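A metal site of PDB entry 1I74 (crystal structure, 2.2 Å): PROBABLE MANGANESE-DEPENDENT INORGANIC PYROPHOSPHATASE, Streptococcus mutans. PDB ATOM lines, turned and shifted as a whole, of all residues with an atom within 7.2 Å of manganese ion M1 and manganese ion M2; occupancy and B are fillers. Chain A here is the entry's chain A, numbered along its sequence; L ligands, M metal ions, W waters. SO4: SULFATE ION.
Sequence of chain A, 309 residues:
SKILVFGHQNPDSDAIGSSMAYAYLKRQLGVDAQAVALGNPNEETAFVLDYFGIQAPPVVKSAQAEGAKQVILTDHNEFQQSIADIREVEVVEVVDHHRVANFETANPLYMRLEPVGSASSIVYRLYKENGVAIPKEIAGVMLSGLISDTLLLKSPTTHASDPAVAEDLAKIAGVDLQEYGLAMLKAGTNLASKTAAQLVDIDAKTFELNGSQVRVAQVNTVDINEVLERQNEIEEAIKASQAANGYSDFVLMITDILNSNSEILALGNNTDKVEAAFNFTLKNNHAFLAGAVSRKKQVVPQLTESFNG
The side-chain carboxylate of Asp 12 lies close to the backbone NH of Ala 15, 2.8 Å away. The backbone NH (N) of His 8 is in hydrogen-bond range of a ring nitrogen (ND1) of His 76, 3.4 Å away. ND1 of His 98 sits at hydrogen-bond distance from OD1 of Asp 96, at 2.6 Å. The side-chain carboxylate (OD1) of Asp 14 lies within hydrogen-bond range of the backbone NH (N) of Ala 119 (3.3 Å). A ring nitrogen (NE2) of His 97 sits close to the backbone NH (N) of Ala 119 (3.5 Å). A ring nitrogen (ND1) of His 97 sits at hydrogen-bond distance from the backbone carbonyl oxygen (O) of Val 116, at 2.9 Å. OD1 of Asp 12 lies close to N of Asp 14. The backbone carbonyl oxygen of Asp 14 sits at hydrogen-bond distance from the side-chain hydroxyl of Ser 18, 2.8 Å away.
Three residues have an atom within 4 Å of manganese ion M1: His 8, Asp 12 and Asp 75.
His 98 touches manganese ion M2 (CE1 to MN, 3.96 Å). Five residues have an atom within 4 Å of manganese ion M2: Asp 14, Asp 75, His 97, His 98 and Asp 149.
Manganese ion M1 is bound by water W1 (1.9 Å), an oxygen (O1) of the ligand (2.0 Å), the side-chain carboxylate (OD2) of Asp 75 (2.1 Å), the side-chain carboxylate (OD2) of Asp 12 (2.1 Å), a ring nitrogen (NE2) of His 8 (2.3 Å) and the side-chain carboxylate (OD1) of Asp 12 (2.5 Å). Manganese ion M1 has six donor atoms within binding distance.
Manganese ion M2 is bound by water W1 (2.1 Å), OD2 of Asp 149 (2.1 Å), OD1 of Asp 75 (2.1 Å), O3 of the ligand (2.1 Å), OD2 of Asp 14 (2.3 Å) and NE2 of His 97 (2.4 Å).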
ATOM      1  N   HIS A   8      27.427  -5.223  -4.514  1.00  0.00           N
ATOM      2  CA  HIS A   8      28.752  -4.648  -4.280  1.00  0.00           C
ATOM      3  C   HIS A   8      29.059  -4.056  -2.908  1.00  0.00           C
ATOM      4  O   HIS A   8      28.185  -3.851  -2.075  1.00  0.00           O
ATOM      5  CB  HIS A   8      29.035  -3.587  -5.340  1.00  0.00           C
ATOM      6  CG  HIS A   8      28.020  -2.482  -5.384  1.00  0.00           C
ATOM      7  ND1 HIS A   8      27.903  -1.544  -4.379  1.00  0.00           N
ATOM      8  CD2 HIS A   8      27.099  -2.165  -6.317  1.00  0.00           C
ATOM      9  CE1 HIS A   8      26.945  -0.692  -4.696  1.00  0.00           C
ATOM     10  NE2 HIS A   8      26.439  -1.039  -5.866  1.00  0.00           N
ATOM     11  N   GLN A   9      30.350  -3.807  -2.686  1.00  0.00           N
ATOM     12  CA  GLN A   9      30.838  -3.199  -1.450  1.00  0.00           C
ATOM     13  C   GLN A   9      30.133  -1.846  -1.371  1.00  0.00           C
ATOM     14  O   GLN A   9      29.786  -1.266  -2.406  1.00  0.00           O
ATOM     15  CB  GLN A   9      32.350  -2.993  -1.529  1.00  0.00           C
ATOM     16  CG  GLN A   9      33.145  -4.285  -1.575  1.00  0.00           C
ATOM     17  CD  GLN A   9      33.251  -4.944  -0.220  1.00  0.00           C
ATOM     18  OE1 GLN A   9      33.806  -6.046  -0.090  1.00  0.00           O
ATOM     19  NE2 GLN A   9      32.745  -4.280   0.812  1.00  0.00           N
ATOM     20  N   ASN A  10      29.955  -1.332  -0.169  1.00  0.00           N
ATOM     21  CA  ASN A  10      29.245  -0.058   0.011  1.00  0.00           C
ATOM     22  C   ASN A  10      27.911  -0.204  -0.713  1.00  0.00           C
ATOM     23  O   ASN A  10      27.559   0.622  -1.549  1.00  0.00           O
ATOM     24  CB  ASN A  10      30.029   1.111  -0.585  1.00  0.00           C
ATOM     25  CG  ASN A  10      31.319   1.373   0.143  1.00  0.00           C
ATOM     26  OD1 ASN A  10      31.529   0.911   1.258  1.00  0.00           O
ATOM     27  ND2 ASN A  10      32.195   2.148  -0.497  1.00  0.00           N
ATOM     28  N   PRO A  11      27.151  -1.256  -0.388  1.00  0.00           N
ATOM     29  CA  PRO A  11      25.847  -1.576  -0.965  1.00  0.00           C
ATOM     30  C   PRO A  11      24.914  -0.372  -1.019  1.00  0.00           C
ATOM     31  O   PRO A  11      24.773   0.342  -0.025  1.00  0.00           O
ATOM     32  CB  PRO A  11      25.283  -2.621  -0.016  1.00  0.00           C
ATOM     33  CG  PRO A  11      26.463  -3.157   0.693  1.00  0.00           C
ATOM     34  CD  PRO A  11      27.376  -2.005   0.853  1.00  0.00           C
ATOM     35  N   ASP A  12      24.279  -0.159  -2.162  1.00  0.00           N
ATOM     36  CA  ASP A  12      23.317   0.919  -2.269  1.00  0.00           C
ATOM     37  C   ASP A  12      21.951   0.233  -2.336  1.00  0.00           C
ATOM     38  O   ASP A  12      21.864  -0.990  -2.166  1.00  0.00           O
ATOM     39  CB  ASP A  12      23.579   1.773  -3.512  1.00  0.00           C
ATOM     40  CG  ASP A  12      23.770   0.947  -4.770  1.00  0.00           C
ATOM     41  OD1 ASP A  12      23.299  -0.213  -4.816  1.00  0.00           O
ATOM     42  OD2 ASP A  12      24.391   1.485  -5.717  1.00  0.00           O
ATOM     43  N   SER A  13      20.880   0.984  -2.557  1.00  0.00           N
ATOM     44  CA  SER A  13      19.560   0.394  -2.588  1.00  0.00           C
ATOM     45  C   SER A  13      19.357  -0.672  -3.668  1.00  0.00           C
ATOM     46  O   SER A  13      18.760  -1.728  -3.410  1.00  0.00           O
ATOM     47  CB  SER A  13      18.502   1.491  -2.749  1.00  0.00           C
ATOM     48  OG  SER A  13      18.429   2.287  -1.585  1.00  0.00           O
ATOM     49  N   ASP A  14      19.862  -0.414  -4.861  1.00  0.00           N
ATOM     50  CA  ASP A  14      19.729  -1.362  -5.952  1.00  0.00           C
ATOM     51  C   ASP A  14      20.493  -2.648  -5.639  1.00  0.00           C
ATOM     52  O   ASP A  14      19.990  -3.746  -5.873  1.00  0.00           O
ATOM     53  CB  ASP A  14      20.225  -0.725  -7.241  1.00  0.00           C
ATOM     54  CG  ASP A  14      19.978  -1.588  -8.460  1.00  0.00           C
ATOM     55  OD1 ASP A  14      18.870  -2.147  -8.583  1.00  0.00           O
ATOM     56  OD2 ASP A  14      20.892  -1.709  -9.288  1.00  0.00           O
ATOM     57  N   ALA A  15      21.689  -2.512  -5.086  1.00  0.00           N
ATOM     58  CA  ALA A  15      22.493  -3.662  -4.738  1.00  0.00           C
ATOM     59  C   ALA A  15      21.756  -4.565  -3.754  1.00  0.00           C
ATOM     60  O   ALA A  15      21.638  -5.770  -3.962  1.00  0.00           O
ATOM     61  CB  ALA A  15      23.820  -3.218  -4.129  1.00  0.00           C
ATOM     62  N   ILE A  16      21.259  -3.968  -2.669  1.00  0.00           N
ATOM     63  CA  ILE A  16      20.540  -4.717  -1.654  1.00  0.00           C
ATOM     64  C   ILE A  16      19.216  -5.260  -2.201  1.00  0.00           C
ATOM     65  O   ILE A  16      18.924  -6.436  -2.060  1.00  0.00           O
ATOM     66  CB  ILE A  16      20.262  -3.841  -0.398  1.00  0.00           C
ATOM     67  CG1 ILE A  16      21.571  -3.407   0.270  1.00  0.00           C
ATOM     68  CG2 ILE A  16      19.436  -4.642   0.623  1.00  0.00           C
ATOM     69  CD1 ILE A  16      22.425  -4.568   0.776  1.00  0.00           C
ATOM     70  N   SER A  18      18.145  -5.779  -5.340  1.00  0.00           N
ATOM     71  CA  SER A  18      18.305  -6.794  -6.368  1.00  0.00           C
ATOM     72  C   SER A  18      18.809  -8.112  -5.779  1.00  0.00           C
ATOM     73  O   SER A  18      18.381  -9.176  -6.204  1.00  0.00           O
ATOM     74  CB  SER A  18      19.260  -6.313  -7.469  1.00  0.00           C
ATOM     75  OG  SER A  18      20.594  -6.194  -7.007  1.00  0.00           O
ATOM     76  N   THR A  74      25.015  -9.611  -7.909  1.00  0.00           N
ATOM     77  CA  THR A  74      23.996  -8.753  -8.507  1.00  0.00           C
ATOM     78  C   THR A  74      24.490  -7.307  -8.430  1.00  0.00           C
ATOM     79  O   THR A  74      25.188  -6.935  -7.485  1.00  0.00           O
ATOM     80  CB  THR A  74      22.610  -8.818  -7.785  1.00  0.00           C
ATOM     81  OG1 THR A  74      22.740  -8.327  -6.448  1.00  0.00           O
ATOM     82  CG2 THR A  74      22.080 -10.235  -7.777  1.00  0.00           C
ATOM     83  N   ASP A  75      24.147  -6.515  -9.446  1.00  0.00           N
ATOM     84  CA  ASP A  75      24.490  -5.109  -9.481  1.00  0.00           C
ATOM     85  C   ASP A  75      25.999  -4.813  -9.541  1.00  0.00           C
ATOM     86  O   ASP A  75      26.435  -3.719  -9.195  1.00  0.00           O
ATOM     87  CB  ASP A  75      23.833  -4.417  -8.278  1.00  0.00           C
ATOM     88  CG  ASP A  75      23.932  -2.908  -8.328  1.00  0.00           C
ATOM     89  OD1 ASP A  75      23.715  -2.325  -9.415  1.00  0.00           O
ATOM     90  OD2 ASP A  75      24.212  -2.297  -7.283  1.00  0.00           O
ATOM     91  N   HIS A  76      26.773  -5.795  -9.977  1.00  0.00           N
ATOM     92  CA  HIS A  76      28.219  -5.648 -10.115  1.00  0.00           C
ATOM     93  C   HIS A  76      28.815  -6.953 -10.614  1.00  0.00           C
ATOM     94  O   HIS A  76      28.207  -8.014 -10.489  1.00  0.00           O
ATOM     95  CB  HIS A  76      28.875  -5.301  -8.782  1.00  0.00           C
ATOM     96  CG  HIS A  76      28.975  -6.464  -7.838  1.00  0.00           C
ATOM     97  ND1 HIS A  76      27.872  -7.085  -7.293  1.00  0.00           N
ATOM     98  CD2 HIS A  76      30.059  -7.116  -7.354  1.00  0.00           C
ATOM     99  CE1 HIS A  76      28.272  -8.078  -6.519  1.00  0.00           C
ATOM    100  NE2 HIS A  76      29.590  -8.124  -6.532  1.00  0.00           N
ATOM    101  N   ASP A  96      23.376  -8.114 -13.612  1.00  0.00           N
ATOM    102  CA  ASP A  96      23.914  -6.783 -13.467  1.00  0.00           C
ATOM    103  C   ASP A  96      23.627  -5.888 -14.668  1.00  0.00           C
ATOM    104  O   ASP A  96      23.221  -6.372 -15.721  1.00  0.00           O
ATOM    105  CB  ASP A  96      25.421  -6.932 -13.220  1.00  0.00           C
ATOM    106  CG  ASP A  96      26.112  -5.621 -12.982  1.00  0.00           C
ATOM    107  OD1 ASP A  96      25.483  -4.711 -12.434  1.00  0.00           O
ATOM    108  OD2 ASP A  96      27.298  -5.519 -13.329  1.00  0.00           O
ATOM    109  N   HIS A  97      23.842  -4.592 -14.508  1.00  0.00           N
ATOM    110  CA  HIS A  97      23.633  -3.646 -15.587  1.00  0.00           C
ATOM    111  C   HIS A  97      24.837  -2.754 -15.837  1.00  0.00           C
ATOM    112  O   HIS A  97      24.705  -1.624 -16.321  1.00  0.00           O
ATOM    113  CB  HIS A  97      22.382  -2.792 -15.339  1.00  0.00           C
ATOM    114  CG  HIS A  97      22.436  -1.950 -14.106  1.00  0.00           C
ATOM    115  ND1 HIS A  97      22.091  -0.620 -14.107  1.00  0.00           N
ATOM    116  CD2 HIS A  97      22.757  -2.255 -12.825  1.00  0.00           C
ATOM    117  CE1 HIS A  97      22.197  -0.145 -12.874  1.00  0.00           C
ATOM    118  NE2 HIS A  97      22.602  -1.116 -12.080  1.00  0.00           N
ATOM    119  N   HIS A  98      26.025  -3.248 -15.501  1.00  0.00           N
ATOM    120  CA  HIS A  98      27.237  -2.495 -15.699  1.00  0.00           C
ATOM    121  C   HIS A  98      28.093  -3.122 -16.783  1.00  0.00           C
ATOM    122  O   HIS A  98      27.856  -4.266 -17.200  1.00  0.00           O
ATOM    123  CB  HIS A  98      28.076  -2.431 -14.428  1.00  0.00           C
ATOM    124  CG  HIS A  98      27.398  -1.723 -13.299  1.00  0.00           C
ATOM    125  ND1 HIS A  98      26.547  -2.369 -12.435  1.00  0.00           N
ATOM    126  CD2 HIS A  98      27.467  -0.437 -12.887  1.00  0.00           C
ATOM    127  CE1 HIS A  98      26.107  -1.510 -11.535  1.00  0.00           C
ATOM    128  NE2 HIS A  98      26.658  -0.328 -11.781  1.00  0.00           N
ATOM    129  N   VAL A 116      20.250  -1.524 -18.746  1.00  0.00           N
ATOM    130  CA  VAL A 116      19.116  -0.771 -18.238  1.00  0.00           C
ATOM    131  C   VAL A 116      19.447   0.051 -17.006  1.00  0.00           C
ATOM    132  O   VAL A 116      20.578   0.058 -16.532  1.00  0.00           O
ATOM    133  CB  VAL A 116      17.933  -1.699 -17.893  1.00  0.00           C
ATOM    134  CG1 VAL A 116      17.382  -2.305 -19.179  1.00  0.00           C
ATOM    135  CG2 VAL A 116      18.368  -2.784 -16.932  1.00  0.00           C
ATOM    136  N   GLY A 117      18.423   0.726 -16.492  1.00  0.00           N
ATOM    137  CA  GLY A 117      18.578   1.597 -15.347  1.00  0.00           C
ATOM    138  C   GLY A 117      18.960   1.019 -13.994  1.00  0.00           C
ATOM    139  O   GLY A 117      19.583   1.721 -13.214  1.00  0.00           O
ATOM    140  N   SER A 118      18.583  -0.223 -13.703  1.00  0.00           N
ATOM    141  CA  SER A 118      18.940  -0.836 -12.424  1.00  0.00           C
ATOM    142  C   SER A 118      18.998  -2.353 -12.543  1.00  0.00           C
ATOM    143  O   SER A 118      18.410  -2.924 -13.460  1.00  0.00           O
ATOM    144  CB  SER A 118      17.929  -0.468 -11.329  1.00  0.00           C
ATOM    145  OG  SER A 118      16.698  -1.162 -11.478  1.00  0.00           O
ATOM    146  N   ALA A 119      19.725  -2.994 -11.635  1.00  0.00           N
ATOM    147  CA  ALA A 119      19.819  -4.443 -11.629  1.00  0.00           C
ATOM    148  C   ALA A 119      18.467  -4.984 -11.190  1.00  0.00           C
ATOM    149  O   ALA A 119      18.058  -6.066 -11.592  1.00  0.00           O
ATOM    150  CB  ALA A 119      20.916  -4.901 -10.680  1.00  0.00           C
ATOM    151  N   SER A 120      17.772  -4.225 -10.347  1.00  0.00           N
ATOM    152  CA  SER A 120      16.458  -4.610  -9.874  1.00  0.00           C
ATOM    153  C   SER A 120      15.488  -4.717 -11.042  1.00  0.00           C
ATOM    154  O   SER A 120      14.597  -5.550 -11.041  1.00  0.00           O
ATOM    155  CB  SER A 120      15.934  -3.586  -8.868  1.00  0.00           C
ATOM    156  OG  SER A 120      16.636  -3.679  -7.645  1.00  0.00           O
ATOM    157  N   GLY A 145      15.219   0.051  -5.538  1.00  0.00           N
ATOM    158  CA  GLY A 145      16.505  -0.045  -6.212  1.00  0.00           C
ATOM    159  C   GLY A 145      16.489   0.736  -7.515  1.00  0.00           C
ATOM    160  O   GLY A 145      17.426   1.466  -7.832  1.00  0.00           O
ATOM    161  N   ASP A 149      18.699   4.171  -8.312  1.00  0.00           N
ATOM    162  CA  ASP A 149      19.648   4.259  -9.410  1.00  0.00           C
ATOM    163  C   ASP A 149      19.295   5.290 -10.480  1.00  0.00           C
ATOM    164  O   ASP A 149      20.186   5.846 -11.115  1.00  0.00           O
ATOM    165  CB  ASP A 149      19.804   2.901 -10.062  1.00  0.00           C
ATOM    166  CG  ASP A 149      20.923   2.074  -9.470  1.00  0.00           C
ATOM    167  OD1 ASP A 149      21.309   2.327  -8.316  1.00  0.00           O
ATOM    168  OD2 ASP A 149      21.410   1.155 -10.160  1.00  0.00           O
ATOM    169  N   ASP A 203      28.795   5.923  -0.704  1.00  0.00           N
ATOM    170  CA  ASP A 203      28.565   5.401  -2.035  1.00  0.00           C
ATOM    171  C   ASP A 203      29.741   5.802  -2.912  1.00  0.00           C
ATOM    172  O   ASP A 203      29.674   6.782  -3.658  1.00  0.00           O
ATOM    173  CB  ASP A 203      27.251   5.978  -2.552  1.00  0.00           C
ATOM    174  CG  ASP A 203      26.871   5.469  -3.904  1.00  0.00           C
ATOM    175  OD1 ASP A 203      27.475   4.488  -4.365  1.00  0.00           O
ATOM    176  OD2 ASP A 203      25.941   6.056  -4.487  1.00  0.00           O
ATOM    177  N   LYS A 205      33.258   4.328  -5.376  1.00  0.00           N
ATOM    178  CA  LYS A 205      33.959   3.290  -6.115  1.00  0.00           C
ATOM    179  C   LYS A 205      35.297   3.829  -6.595  1.00  0.00           C
ATOM    180  O   LYS A 205      35.498   5.048  -6.628  1.00  0.00           O
ATOM    181  CB  LYS A 205      33.147   2.838  -7.338  1.00  0.00           C
ATOM    182  CG  LYS A 205      31.775   2.341  -7.014  1.00  0.00           C
ATOM    183  CD  LYS A 205      31.038   1.786  -8.245  1.00  0.00           C
ATOM    184  CE  LYS A 205      30.634   2.884  -9.222  1.00  0.00           C
ATOM    185  NZ  LYS A 205      29.558   2.430 -10.160  1.00  0.00           N
ATOM    186  N   ARG A 295      26.763   9.607 -11.787  1.00  0.00           N
ATOM    187  CA  ARG A 295      28.197   9.465 -11.752  1.00  0.00           C
ATOM    188  C   ARG A 295      28.672   8.742 -13.011  1.00  0.00           C
ATOM    189  O   ARG A 295      29.529   9.251 -13.732  1.00  0.00           O
ATOM    190  CB  ARG A 295      28.646   8.701 -10.499  1.00  0.00           C
ATOM    191  CG  ARG A 295      30.135   8.343 -10.465  1.00  0.00           C
ATOM    192  CD  ARG A 295      30.563   7.740  -9.126  1.00  0.00           C
ATOM    193  NE  ARG A 295      29.711   6.619  -8.732  1.00  0.00           N
ATOM    194  CZ  ARG A 295      29.538   6.208  -7.470  1.00  0.00           C
ATOM    195  NH1 ARG A 295      30.170   6.827  -6.476  1.00  0.00           N
ATOM    196  NH2 ARG A 295      28.721   5.199  -7.204  1.00  0.00           N
ATOM    197  N   LYS A 296      28.082   7.582 -13.297  1.00  0.00           N
ATOM    198  CA  LYS A 296      28.510   6.795 -14.461  1.00  0.00           C
ATOM    199  C   LYS A 296      28.359   7.479 -15.812  1.00  0.00           C
ATOM    200  O   LYS A 296      29.165   7.244 -16.715  1.00  0.00           O
ATOM    201  CB  LYS A 296      27.786   5.446 -14.502  1.00  0.00           C
ATOM    202  CG  LYS A 296      26.310   5.504 -14.895  1.00  0.00           C
ATOM    203  CD  LYS A 296      25.670   4.116 -14.852  1.00  0.00           C
ATOM    204  CE  LYS A 296      26.347   3.110 -15.807  1.00  0.00           C
ATOM    205  NZ  LYS A 296      25.884   1.696 -15.557  1.00  0.00           N
HETATM  206  S   SO4 L   1      25.364   1.479  -9.487  1.00  0.00           S
HETATM  207  O1  SO4 L   1      25.685   0.627  -8.342  1.00  0.00           O
HETATM  208  O2  SO4 L   1      26.601   1.808 -10.233  1.00  0.00           O
HETATM  209  O3  SO4 L   1      24.412   0.757 -10.364  1.00  0.00           O
HETATM  210  O4  SO4 L   1      24.746   2.711  -8.991  1.00  0.00           O
HETATM  211 MN    MN M   1      24.566  -0.238  -6.989  1.00  0.00          MN
HETATM  212 MN    MN M   2      22.744  -0.448  -9.743  1.00  0.00          MN
HETATM  213 MG    MG M   3      24.942   4.481  -8.292  1.00  0.00          MG
HETATM  214  O   HOH W   1      22.905   0.262  -7.797  1.00  0.00           O
